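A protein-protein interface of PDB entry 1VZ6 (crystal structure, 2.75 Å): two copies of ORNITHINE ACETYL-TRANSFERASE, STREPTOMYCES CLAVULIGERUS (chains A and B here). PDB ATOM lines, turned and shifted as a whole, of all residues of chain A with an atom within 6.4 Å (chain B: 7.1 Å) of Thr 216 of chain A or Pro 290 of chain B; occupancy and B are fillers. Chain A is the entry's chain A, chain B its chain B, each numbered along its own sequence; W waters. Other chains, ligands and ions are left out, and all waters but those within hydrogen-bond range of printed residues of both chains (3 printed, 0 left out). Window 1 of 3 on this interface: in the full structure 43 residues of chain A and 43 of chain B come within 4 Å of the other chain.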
ATOM      1  N   MET A 174     -15.616 -27.969 -10.101  1.00  0.00           N
ATOM      2  CA  MET A 174     -15.439 -26.680  -9.422  1.00  0.00           C
ATOM      3  C   MET A 174     -16.367 -25.767 -10.208  1.00  0.00           C
ATOM      4  O   MET A 174     -15.987 -24.682 -10.651  1.00  0.00           O
ATOM      5  CB  MET A 174     -13.998 -26.180  -9.529  1.00  0.00           C
ATOM      6  CG  MET A 174     -13.689 -25.049  -8.559  1.00  0.00           C
ATOM      7  SD  MET A 174     -12.109 -24.234  -8.854  1.00  0.00           S
ATOM      8  CE  MET A 174     -10.988 -25.389  -8.067  1.00  0.00           C
ATOM      9  N   LEU A 175     -17.605 -26.219 -10.361  1.00  0.00           N
ATOM     10  CA  LEU A 175     -18.541 -25.480 -11.171  1.00  0.00           C
ATOM     11  C   LEU A 175     -19.959 -25.212 -10.681  1.00  0.00           C
ATOM     12  O   LEU A 175     -20.823 -26.092 -10.668  1.00  0.00           O
ATOM     13  CB  LEU A 175     -18.594 -26.149 -12.544  1.00  0.00           C
ATOM     14  CG  LEU A 175     -19.162 -25.317 -13.686  1.00  0.00           C
ATOM     15  CD1 LEU A 175     -18.360 -25.608 -14.930  1.00  0.00           C
ATOM     16  CD2 LEU A 175     -20.641 -25.615 -13.891  1.00  0.00           C
ATOM     17  N   GLU A 176     -20.162 -23.968 -10.276  1.00  0.00           N
ATOM     18  CA  GLU A 176     -21.449 -23.428  -9.856  1.00  0.00           C
ATOM     19  C   GLU A 176     -21.234 -21.918  -9.912  1.00  0.00           C
ATOM     20  O   GLU A 176     -21.104 -21.249  -8.887  1.00  0.00           O
ATOM     21  CB  GLU A 176     -21.862 -23.846  -8.443  1.00  0.00           C
ATOM     22  CG  GLU A 176     -23.099 -23.058  -8.008  1.00  0.00           C
ATOM     23  CD  GLU A 176     -23.946 -23.727  -6.953  1.00  0.00           C
ATOM     24  OE1 GLU A 176     -23.415 -24.051  -5.859  1.00  0.00           O
ATOM     25  OE2 GLU A 176     -25.157 -23.915  -7.218  1.00  0.00           O
ATOM     26  N   SER A 213     -24.974 -26.105 -11.814  1.00  0.00           N
ATOM     27  CA  SER A 213     -24.114 -26.500 -10.713  1.00  0.00           C
ATOM     28  C   SER A 213     -23.721 -27.969 -10.771  1.00  0.00           C
ATOM     29  O   SER A 213     -24.571 -28.857 -10.772  1.00  0.00           O
ATOM     30  CB  SER A 213     -24.795 -26.227  -9.382  1.00  0.00           C
ATOM     31  OG  SER A 213     -24.022 -26.762  -8.321  1.00  0.00           O
ATOM     32  N   ILE A 214     -22.422 -28.223 -10.821  1.00  0.00           N
ATOM     33  CA  ILE A 214     -21.934 -29.590 -10.839  1.00  0.00           C
ATOM     34  C   ILE A 214     -21.660 -30.003  -9.387  1.00  0.00           C
ATOM     35  O   ILE A 214     -22.312 -30.897  -8.858  1.00  0.00           O
ATOM     36  CB  ILE A 214     -20.620 -29.715 -11.650  1.00  0.00           C
ATOM     37  CG1 ILE A 214     -20.835 -29.271 -13.102  1.00  0.00           C
ATOM     38  CG2 ILE A 214     -20.123 -31.147 -11.602  1.00  0.00           C
ATOM     39  CD1 ILE A 214     -21.658 -30.224 -13.933  1.00  0.00           C
ATOM     40  N   ASP A 215     -20.718 -29.322  -8.737  1.00  0.00           N
ATOM     41  CA  ASP A 215     -20.343 -29.658  -7.358  1.00  0.00           C
ATOM     42  C   ASP A 215     -20.502 -28.556  -6.309  1.00  0.00           C
ATOM     43  O   ASP A 215     -20.021 -28.705  -5.186  1.00  0.00           O
ATOM     44  CB  ASP A 215     -18.889 -30.132  -7.326  1.00  0.00           C
ATOM     45  CG  ASP A 215     -17.966 -29.210  -8.102  1.00  0.00           C
ATOM     46  OD1 ASP A 215     -18.217 -27.980  -8.118  1.00  0.00           O
ATOM     47  OD2 ASP A 215     -16.983 -29.716  -8.691  1.00  0.00           O
ATOM     48  N   THR A 216     -21.169 -27.466  -6.683  1.00  0.00           N
ATOM     49  CA  THR A 216     -21.403 -26.306  -5.815  1.00  0.00           C
ATOM     50  C   THR A 216     -20.140 -25.506  -5.532  1.00  0.00           C
ATOM     51  O   THR A 216     -20.197 -24.506  -4.823  1.00  0.00           O
ATOM     52  CB  THR A 216     -22.006 -26.677  -4.415  1.00  0.00           C
ATOM     53  OG1 THR A 216     -20.947 -26.953  -3.486  1.00  0.00           O
ATOM     54  CG2 THR A 216     -22.943 -27.877  -4.510  1.00  0.00           C
ATOM     55  N   ASP A 217     -19.005 -25.927  -6.082  1.00  0.00           N
ATOM     56  CA  ASP A 217     -17.754 -25.226  -5.811  1.00  0.00           C
ATOM     57  C   ASP A 217     -17.450 -24.055  -6.730  1.00  0.00           C
ATOM     58  O   ASP A 217     -16.667 -24.172  -7.667  1.00  0.00           O
ATOM     59  CB  ASP A 217     -16.581 -26.211  -5.816  1.00  0.00           C
ATOM     60  CG  ASP A 217     -16.574 -27.115  -4.585  1.00  0.00           C
ATOM     61  OD1 ASP A 217     -16.826 -26.606  -3.471  1.00  0.00           O
ATOM     62  OD2 ASP A 217     -16.308 -28.330  -4.728  1.00  0.00           O
ATOM     63  N   THR A 218     -18.063 -22.915  -6.433  1.00  0.00           N
ATOM     64  CA  THR A 218     -17.867 -21.717  -7.225  1.00  0.00           C
ATOM     65  C   THR A 218     -16.390 -21.432  -7.350  1.00  0.00           C
ATOM     66  O   THR A 218     -15.692 -21.276  -6.353  1.00  0.00           O
ATOM     67  CB  THR A 218     -18.541 -20.527  -6.579  1.00  0.00           C
ATOM     68  OG1 THR A 218     -19.920 -20.837  -6.370  1.00  0.00           O
ATOM     69  CG2 THR A 218     -18.435 -19.310  -7.474  1.00  0.00           C
ATOM     70  N   ASN A 288     -28.273 -29.820  -5.940  1.00  0.00           N
ATOM     71  CA  ASN A 288     -26.997 -29.934  -5.239  1.00  0.00           C
ATOM     72  C   ASN A 288     -27.054 -30.941  -4.097  1.00  0.00           C
ATOM     73  O   ASN A 288     -26.042 -31.192  -3.427  1.00  0.00           O
ATOM     74  CB  ASN A 288     -26.550 -28.584  -4.690  1.00  0.00           C
ATOM     75  CG  ASN A 288     -26.017 -27.670  -5.763  1.00  0.00           C
ATOM     76  OD1 ASN A 288     -25.233 -28.089  -6.617  1.00  0.00           O
ATOM     77  ND2 ASN A 288     -26.429 -26.409  -5.723  1.00  0.00           N
ATOM     78  N   LYS A 293     -28.667 -36.472  -6.057  1.00  0.00           N
ATOM     79  CA  LYS A 293     -27.719 -36.755  -7.124  1.00  0.00           C
ATOM     80  C   LYS A 293     -27.410 -38.247  -7.205  1.00  0.00           C
ATOM     81  O   LYS A 293     -27.370 -38.805  -8.299  1.00  0.00           O
ATOM     82  CB  LYS A 293     -26.420 -35.969  -6.907  1.00  0.00           C
ATOM     83  CG  LYS A 293     -26.539 -34.443  -7.060  1.00  0.00           C
ATOM     84  CD  LYS A 293     -25.276 -33.738  -6.546  1.00  0.00           C
ATOM     85  CE  LYS A 293     -24.473 -33.063  -7.650  1.00  0.00           C
ATOM     86  NZ  LYS A 293     -23.975 -34.002  -8.690  1.00  0.00           N
ATOM     87  N   TYR A 384     -16.609 -39.089 -10.122  1.00  0.00           N
ATOM     88  CA  TYR A 384     -16.282 -37.801  -9.529  1.00  0.00           C
ATOM     89  C   TYR A 384     -15.268 -37.995  -8.415  1.00  0.00           C
ATOM     90  O   TYR A 384     -14.271 -37.281  -8.344  1.00  0.00           O
ATOM     91  CB  TYR A 384     -17.538 -37.118  -8.970  1.00  0.00           C
ATOM     92  CG  TYR A 384     -17.274 -35.717  -8.448  1.00  0.00           C
ATOM     93  CD1 TYR A 384     -16.760 -35.511  -7.170  1.00  0.00           C
ATOM     94  CD2 TYR A 384     -17.482 -34.601  -9.265  1.00  0.00           C
ATOM     95  CE1 TYR A 384     -16.451 -34.225  -6.717  1.00  0.00           C
ATOM     96  CE2 TYR A 384     -17.179 -33.317  -8.827  1.00  0.00           C
ATOM     97  CZ  TYR A 384     -16.661 -33.132  -7.552  1.00  0.00           C
ATOM     98  OH  TYR A 384     -16.336 -31.862  -7.129  1.00  0.00           O
ATOM     99  N   ASN A 388     -11.299 -36.732  -8.596  1.00  0.00           N
ATOM    100  CA  ASN A 388     -10.886 -35.749  -7.601  1.00  0.00           C
ATOM    101  C   ASN A 388     -10.126 -36.262  -6.387  1.00  0.00           C
ATOM    102  O   ASN A 388      -9.639 -35.470  -5.580  1.00  0.00           O
ATOM    103  CB  ASN A 388     -12.103 -34.926  -7.182  1.00  0.00           C
ATOM    104  CG  ASN A 388     -12.668 -34.121  -8.338  1.00  0.00           C
ATOM    105  OD1 ASN A 388     -11.973 -33.281  -8.917  1.00  0.00           O
ATOM    106  ND2 ASN A 388     -13.925 -34.385  -8.696  1.00  0.00           N
ATOM    107  N   THR B 216     -24.697 -32.542   3.953  1.00  0.00           N
ATOM    108  CA  THR B 216     -25.455 -31.278   3.902  1.00  0.00           C
ATOM    109  C   THR B 216     -26.966 -31.477   3.812  1.00  0.00           C
ATOM    110  O   THR B 216     -27.718 -30.500   3.760  1.00  0.00           O
ATOM    111  CB  THR B 216     -25.072 -30.359   2.688  1.00  0.00           C
ATOM    112  OG1 THR B 216     -25.870 -30.714   1.544  1.00  0.00           O
ATOM    113  CG2 THR B 216     -23.584 -30.475   2.348  1.00  0.00           C
ATOM    114  N   THR B 285     -18.743 -24.263   4.883  1.00  0.00           N
ATOM    115  CA  THR B 285     -18.498 -24.241   3.449  1.00  0.00           C
ATOM    116  C   THR B 285     -17.313 -25.121   3.097  1.00  0.00           C
ATOM    117  O   THR B 285     -17.346 -25.847   2.109  1.00  0.00           O
ATOM    118  CB  THR B 285     -18.243 -22.812   2.932  1.00  0.00           C
ATOM    119  OG1 THR B 285     -19.427 -22.024   3.111  1.00  0.00           O
ATOM    120  CG2 THR B 285     -17.884 -22.830   1.446  1.00  0.00           C
ATOM    121  N   VAL B 286     -16.266 -25.068   3.910  1.00  0.00           N
ATOM    122  CA  VAL B 286     -15.090 -25.886   3.646  1.00  0.00           C
ATOM    123  C   VAL B 286     -15.353 -27.377   3.832  1.00  0.00           C
ATOM    124  O   VAL B 286     -14.999 -28.173   2.974  1.00  0.00           O
ATOM    125  CB  VAL B 286     -13.906 -25.484   4.543  1.00  0.00           C
ATOM    126  CG1 VAL B 286     -12.727 -26.441   4.310  1.00  0.00           C
ATOM    127  CG2 VAL B 286     -13.505 -24.054   4.246  1.00  0.00           C
ATOM    128  N   VAL B 287     -15.981 -27.751   4.942  1.00  0.00           N
ATOM    129  CA  VAL B 287     -16.239 -29.158   5.215  1.00  0.00           C
ATOM    130  C   VAL B 287     -17.297 -29.783   4.293  1.00  0.00           C
ATOM    131  O   VAL B 287     -17.379 -31.006   4.184  1.00  0.00           O
ATOM    132  CB  VAL B 287     -16.644 -29.371   6.710  1.00  0.00           C
ATOM    133  CG1 VAL B 287     -18.138 -29.100   6.909  1.00  0.00           C
ATOM    134  CG2 VAL B 287     -16.279 -30.772   7.152  1.00  0.00           C
ATOM    135  N   ASN B 288     -18.098 -28.951   3.633  1.00  0.00           N
ATOM    136  CA  ASN B 288     -19.125 -29.448   2.716  1.00  0.00           C
ATOM    137  C   ASN B 288     -18.694 -29.366   1.254  1.00  0.00           C
ATOM    138  O   ASN B 288     -19.429 -29.785   0.361  1.00  0.00           O
ATOM    139  CB  ASN B 288     -20.432 -28.680   2.889  1.00  0.00           C
ATOM    140  CG  ASN B 288     -21.167 -29.073   4.141  1.00  0.00           C
ATOM    141  OD1 ASN B 288     -21.280 -30.252   4.451  1.00  0.00           O
ATOM    142  ND2 ASN B 288     -21.684 -28.092   4.865  1.00  0.00           N
ATOM    143  N   SER B 289     -17.501 -28.830   1.016  1.00  0.00           N
ATOM    144  CA  SER B 289     -16.975 -28.707  -0.336  1.00  0.00           C
ATOM    145  C   SER B 289     -16.556 -30.059  -0.902  1.00  0.00           C
ATOM    146  O   SER B 289     -15.573 -30.648  -0.450  1.00  0.00           O
ATOM    147  CB  SER B 289     -15.770 -27.766  -0.351  1.00  0.00           C
ATOM    148  OG  SER B 289     -15.078 -27.846  -1.588  1.00  0.00           O
ATOM    149  N   PRO B 290     -17.300 -30.566  -1.907  1.00  0.00           N
ATOM    150  CA  PRO B 290     -16.995 -31.857  -2.539  1.00  0.00           C
ATOM    151  C   PRO B 290     -15.529 -31.967  -2.965  1.00  0.00           C
ATOM    152  O   PRO B 290     -14.916 -33.029  -2.833  1.00  0.00           O
ATOM    153  CB  PRO B 290     -17.943 -31.889  -3.732  1.00  0.00           C
ATOM    154  CG  PRO B 290     -19.126 -31.140  -3.221  1.00  0.00           C
ATOM    155  CD  PRO B 290     -18.502 -29.962  -2.514  1.00  0.00           C
ATOM    156  N   LEU B 291     -14.963 -30.873  -3.469  1.00  0.00           N
ATOM    157  CA  LEU B 291     -13.570 -30.900  -3.883  1.00  0.00           C
ATOM    158  C   LEU B 291     -12.610 -31.019  -2.693  1.00  0.00           C
ATOM    159  O   LEU B 291     -11.520 -31.580  -2.818  1.00  0.00           O
ATOM    160  CB  LEU B 291     -13.240 -29.663  -4.724  1.00  0.00           C
ATOM    161  CG  LEU B 291     -13.721 -29.728  -6.176  1.00  0.00           C
ATOM    162  CD1 LEU B 291     -13.351 -28.448  -6.885  1.00  0.00           C
ATOM    163  CD2 LEU B 291     -13.099 -30.920  -6.878  1.00  0.00           C
ATOM    164  N   VAL B 292     -13.012 -30.493  -1.539  1.00  0.00           N
ATOM    165  CA  VAL B 292     -12.165 -30.605  -0.356  1.00  0.00           C
ATOM    166  C   VAL B 292     -12.307 -32.020   0.218  1.00  0.00           C
ATOM    167  O   VAL B 292     -11.312 -32.667   0.572  1.00  0.00           O
ATOM    168  CB  VAL B 292     -12.552 -29.566   0.725  1.00  0.00           C
ATOM    169  CG1 VAL B 292     -11.742 -29.803   1.994  1.00  0.00           C
ATOM    170  CG2 VAL B 292     -12.300 -28.162   0.196  1.00  0.00           C
ATOM    171  N   LYS B 293     -13.549 -32.495   0.288  1.00  0.00           N
ATOM    172  CA  LYS B 293     -13.845 -33.828   0.808  1.00  0.00           C
ATOM    173  C   LYS B 293     -13.108 -34.915   0.022  1.00  0.00           C
ATOM    174  O   LYS B 293     -12.556 -35.842   0.613  1.00  0.00           O
ATOM    175  CB  LYS B 293     -15.352 -34.094   0.765  1.00  0.00           C
ATOM    176  CG  LYS B 293     -16.197 -33.251   1.727  1.00  0.00           C
ATOM    177  CD  LYS B 293     -17.687 -33.383   1.413  1.00  0.00           C
ATOM    178  CE  LYS B 293     -18.463 -34.102   2.503  1.00  0.00           C
ATOM    179  NZ  LYS B 293     -18.035 -35.507   2.747  1.00  0.00           N
ATOM    180  N   THR B 294     -13.093 -34.802  -1.305  1.00  0.00           N
ATOM    181  CA  THR B 294     -12.410 -35.790  -2.137  1.00  0.00           C
ATOM    182  C   THR B 294     -10.910 -35.673  -1.979  1.00  0.00           C
ATOM    183  O   THR B 294     -10.208 -36.679  -1.945  1.00  0.00           O
ATOM    184  CB  THR B 294     -12.746 -35.626  -3.625  1.00  0.00           C
ATOM    185  OG1 THR B 294     -12.728 -34.237  -3.957  1.00  0.00           O
ATOM    186  CG2 THR B 294     -14.109 -36.219  -3.942  1.00  0.00           C
ATOM    187  N   ALA B 295     -10.420 -34.441  -1.888  1.00  0.00           N
ATOM    188  CA  ALA B 295      -8.992 -34.214  -1.721  1.00  0.00           C
ATOM    189  C   ALA B 295      -8.512 -34.943  -0.476  1.00  0.00           C
ATOM    190  O   ALA B 295      -7.561 -35.714  -0.528  1.00  0.00           O
ATOM    191  CB  ALA B 295      -8.710 -32.730  -1.595  1.00  0.00           C
ATOM    192  N   VAL B 296      -9.184 -34.698   0.642  1.00  0.00           N
ATOM    193  CA  VAL B 296      -8.828 -35.340   1.901  1.00  0.00           C
ATOM    194  C   VAL B 296      -8.885 -36.866   1.798  1.00  0.00           C
ATOM    195  O   VAL B 296      -8.151 -37.569   2.494  1.00  0.00           O
ATOM    196  CB  VAL B 296      -9.759 -34.859   3.047  1.00  0.00           C
ATOM    197  CG1 VAL B 296      -9.570 -35.718   4.289  1.00  0.00           C
ATOM    198  CG2 VAL B 296      -9.458 -33.407   3.371  1.00  0.00           C
ATOM    199  N   ARG B 305      -7.759 -26.110  -2.784  1.00  0.00           N
ATOM    200  CA  ARG B 305      -9.191 -26.331  -2.771  1.00  0.00           C
ATOM    201  C   ARG B 305      -9.837 -25.704  -1.531  1.00  0.00           C
ATOM    202  O   ARG B 305     -10.976 -25.236  -1.592  1.00  0.00           O
ATOM    203  CB  ARG B 305      -9.487 -27.825  -2.866  1.00  0.00           C
ATOM    204  CG  ARG B 305      -9.141 -28.409  -4.216  1.00  0.00           C
ATOM    205  CD  ARG B 305      -9.456 -29.881  -4.279  1.00  0.00           C
ATOM    206  NE  ARG B 305      -9.252 -30.422  -5.619  1.00  0.00           N
ATOM    207  CZ  ARG B 305      -9.478 -31.691  -5.958  1.00  0.00           C
ATOM    208  NH1 ARG B 305      -9.919 -32.568  -5.055  1.00  0.00           N
ATOM    209  NH2 ARG B 305      -9.267 -32.085  -7.206  1.00  0.00           N
ATOM    210  N   MET B 308     -10.248 -22.103  -2.375  1.00  0.00           N
ATOM    211  CA  MET B 308     -11.392 -21.978  -3.271  1.00  0.00           C
ATOM    212  C   MET B 308     -12.676 -22.020  -2.432  1.00  0.00           C
ATOM    213  O   MET B 308     -13.593 -21.214  -2.629  1.00  0.00           O
ATOM    214  CB  MET B 308     -11.378 -23.137  -4.280  1.00  0.00           C
ATOM    215  CG  MET B 308     -12.622 -23.295  -5.168  1.00  0.00           C
ATOM    216  SD  MET B 308     -14.047 -24.032  -4.342  1.00  0.00           S
ATOM    217  CE  MET B 308     -13.399 -25.716  -3.942  1.00  0.00           C
ATOM    218  N   LYS B 312     -15.743 -19.068  -1.628  1.00  0.00           N
ATOM    219  CA  LYS B 312     -17.160 -19.184  -1.990  1.00  0.00           C
ATOM    220  C   LYS B 312     -18.054 -18.304  -1.113  1.00  0.00           C
ATOM    221  O   LYS B 312     -19.199 -18.036  -1.463  1.00  0.00           O
ATOM    222  CB  LYS B 312     -17.632 -20.645  -1.915  1.00  0.00           C
ATOM    223  CG  LYS B 312     -16.951 -21.564  -2.917  1.00  0.00           C
ATOM    224  CD  LYS B 312     -17.707 -22.868  -3.111  1.00  0.00           C
ATOM    225  CE  LYS B 312     -17.841 -23.649  -1.821  1.00  0.00           C
ATOM    226  NZ  LYS B 312     -18.585 -24.925  -2.025  1.00  0.00           N
ATOM    227  N   LEU B 380     -15.313 -37.575   1.140  1.00  0.00           N
ATOM    228  CA  LEU B 380     -16.299 -38.126   0.220  1.00  0.00           C
ATOM    229  C   LEU B 380     -15.662 -39.323  -0.468  1.00  0.00           C
ATOM    230  O   LEU B 380     -14.566 -39.219  -1.013  1.00  0.00           O
ATOM    231  CB  LEU B 380     -16.701 -37.074  -0.808  1.00  0.00           C
ATOM    232  CG  LEU B 380     -17.628 -37.524  -1.937  1.00  0.00           C
ATOM    233  CD1 LEU B 380     -18.899 -38.093  -1.359  1.00  0.00           C
ATOM    234  CD2 LEU B 380     -17.932 -36.342  -2.856  1.00  0.00           C
HETATM  235  O   HOH W   1     -21.507 -27.903  -0.967  1.00  0.00           O
HETATM  236  O   HOH W   2     -25.397 -29.139  -1.071  1.00  0.00           O
HETATM  237  O   HOH W   3     -21.217 -23.560  -1.838  1.00  0.00           O
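3 positions are printed for both chains. Of the 18 pairs that touch across the chains among the printed residues, none has its exchanged pair printed and touching as well.
Water W1 lies within hydrogen-bond range of OG1 of Thr 216 of chain A and O of Asn 288 of chain B. Water W3 lies within hydrogen-bond range of NZ of Lys 312 of chain B and O of Thr 216 of chain A. Water W2 bridges OG1 of Thr 216 of chain B (3.1 Å) and O of Asn 288 of chain A (3.2 Å).
Of the printed residues of chain B, Thr 216 of chain A touches Pro 290 and Lys 312. Of the printed residues of chain A, Pro 290 of chain B touches Asp 215 (3.3 Å), Thr 216 (3.997 Å), Asp 217 (3.5 Å) and Tyr 384 (3.8 Å). Of the printed residues of chain A, Thr 294 of chain B touches Asn 388. Of the printed residues of chain A, Ser 289 of chain B touches Asp 217. Of the printed residues of chain B, Tyr 384 of chain A touches Pro 290 and Leu 291. Printed residues of chain B within 4 Å of Asp 215 of chain A: Pro 290. Leu 380 of chain B touches none of the printed residues of chain A. The nearest printed residue of chain B that does not touch Asp 217 of chain A is Val 292 of chain B (5.1 Å).
Among the printed residues, merely in contact across the chains: Met 174 of chain A with Leu 291 of chain B, Met 174 of chain A with Met 308 of chain B, Asp 215 of chain A with Pro 290 of chain B, Thr 216 of chain A with Pro 290 of chain B, Asp 217 of chain A with Pro 290 of chain B, Asp 217 of chain A with Met 308 of chain B, Thr 218 of chain A with Lys 312 of chain B, Tyr 384 of chain A with Pro 290 of chain B, Tyr 384 of chain A with Leu 291 of chain B, Asn 388 of chain A with Leu 291 of chain B, Asn 388 of chain A with Thr 294 of chain B and Asn 388 of chain A with Ala 295 of chain B.
Printed residues of chain B that touch a printed residue of chain A: Ser 289, Pro 290, Leu 291, Thr 294, Ala 295, Arg 305, Met 308 and Lys 312. Printed residues of chain A that touch a printed residue of chain B: Met 174, Asp 215, Thr 216, Asp 217, Thr 218, Tyr 384 and Asn 388. Hydrophobic or aromatic side chains of chain A that line the printed part of chain B: Met 174 and Tyr 384. Among the printed residues, Asp or Glu carboxylates within 4 Å of a Lys or Arg side-chain nitrogen of the other chain: Asp 217 of chain A with Lys 312 of chain B (2.8 Å).
The backbone NH of Met 174 of chain A lies within hydrogen-bond range of the side-chain carboxylate of Asp 215 of chain A. The backbone NH (N) of Leu 175 of chain A lies within hydrogen-bond range of the side-chain carboxylate (OD1) of Asp 215 of chain A. The side-chain hydroxyl (OH) of Tyr 384 of chain A is in hydrogen-bond range of the side-chain carboxylate (OD2) of Asp 215 of chain A (2.7 Å). O of Tyr 384 of chain A lies within hydrogen-bond range of ND2 of Asn 388 of chain A. The side-chain hydroxyl (OG) of Ser 289 of chain B sits close to the backbone NH (N) of Val 292 of chain B (3.4 Å). The backbone carbonyl oxygen (O) of Leu 291 of chain B lies within hydrogen-bond range of the guanidinium group (NH1) of Arg 305 of chain B (2.9 Å).
The backbone carbonyl oxygen (O) of Thr 216 of chain A sits at hydrogen-bond distance from the side-chain amino group (NZ) of Lys 312 of chain B (3.3 Å). The side-chain carboxylate (OD1) of Asp 217 of chain A is in hydrogen-bond range of the side-chain hydroxyl (OG) of Ser 289 of chain B (2.9 Å). OD2 of Asp 217 of chain A sits at hydrogen-bond distance from N of Leu 291 of chain B, at 3.1 Å. NZ of Lys 312 of chain B lies within salt-bridge range of OD1 of Asp 217 of chain A (2.8 Å). O of Asn 388 of chain A sits at hydrogen-bond distance from NH1 of Arg 305 of chain B. The side-chain sulfur of Met 308 of chain B lies close to the backbone carbonyl oxygen of Thr 218 of chain A (3.8 Å).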
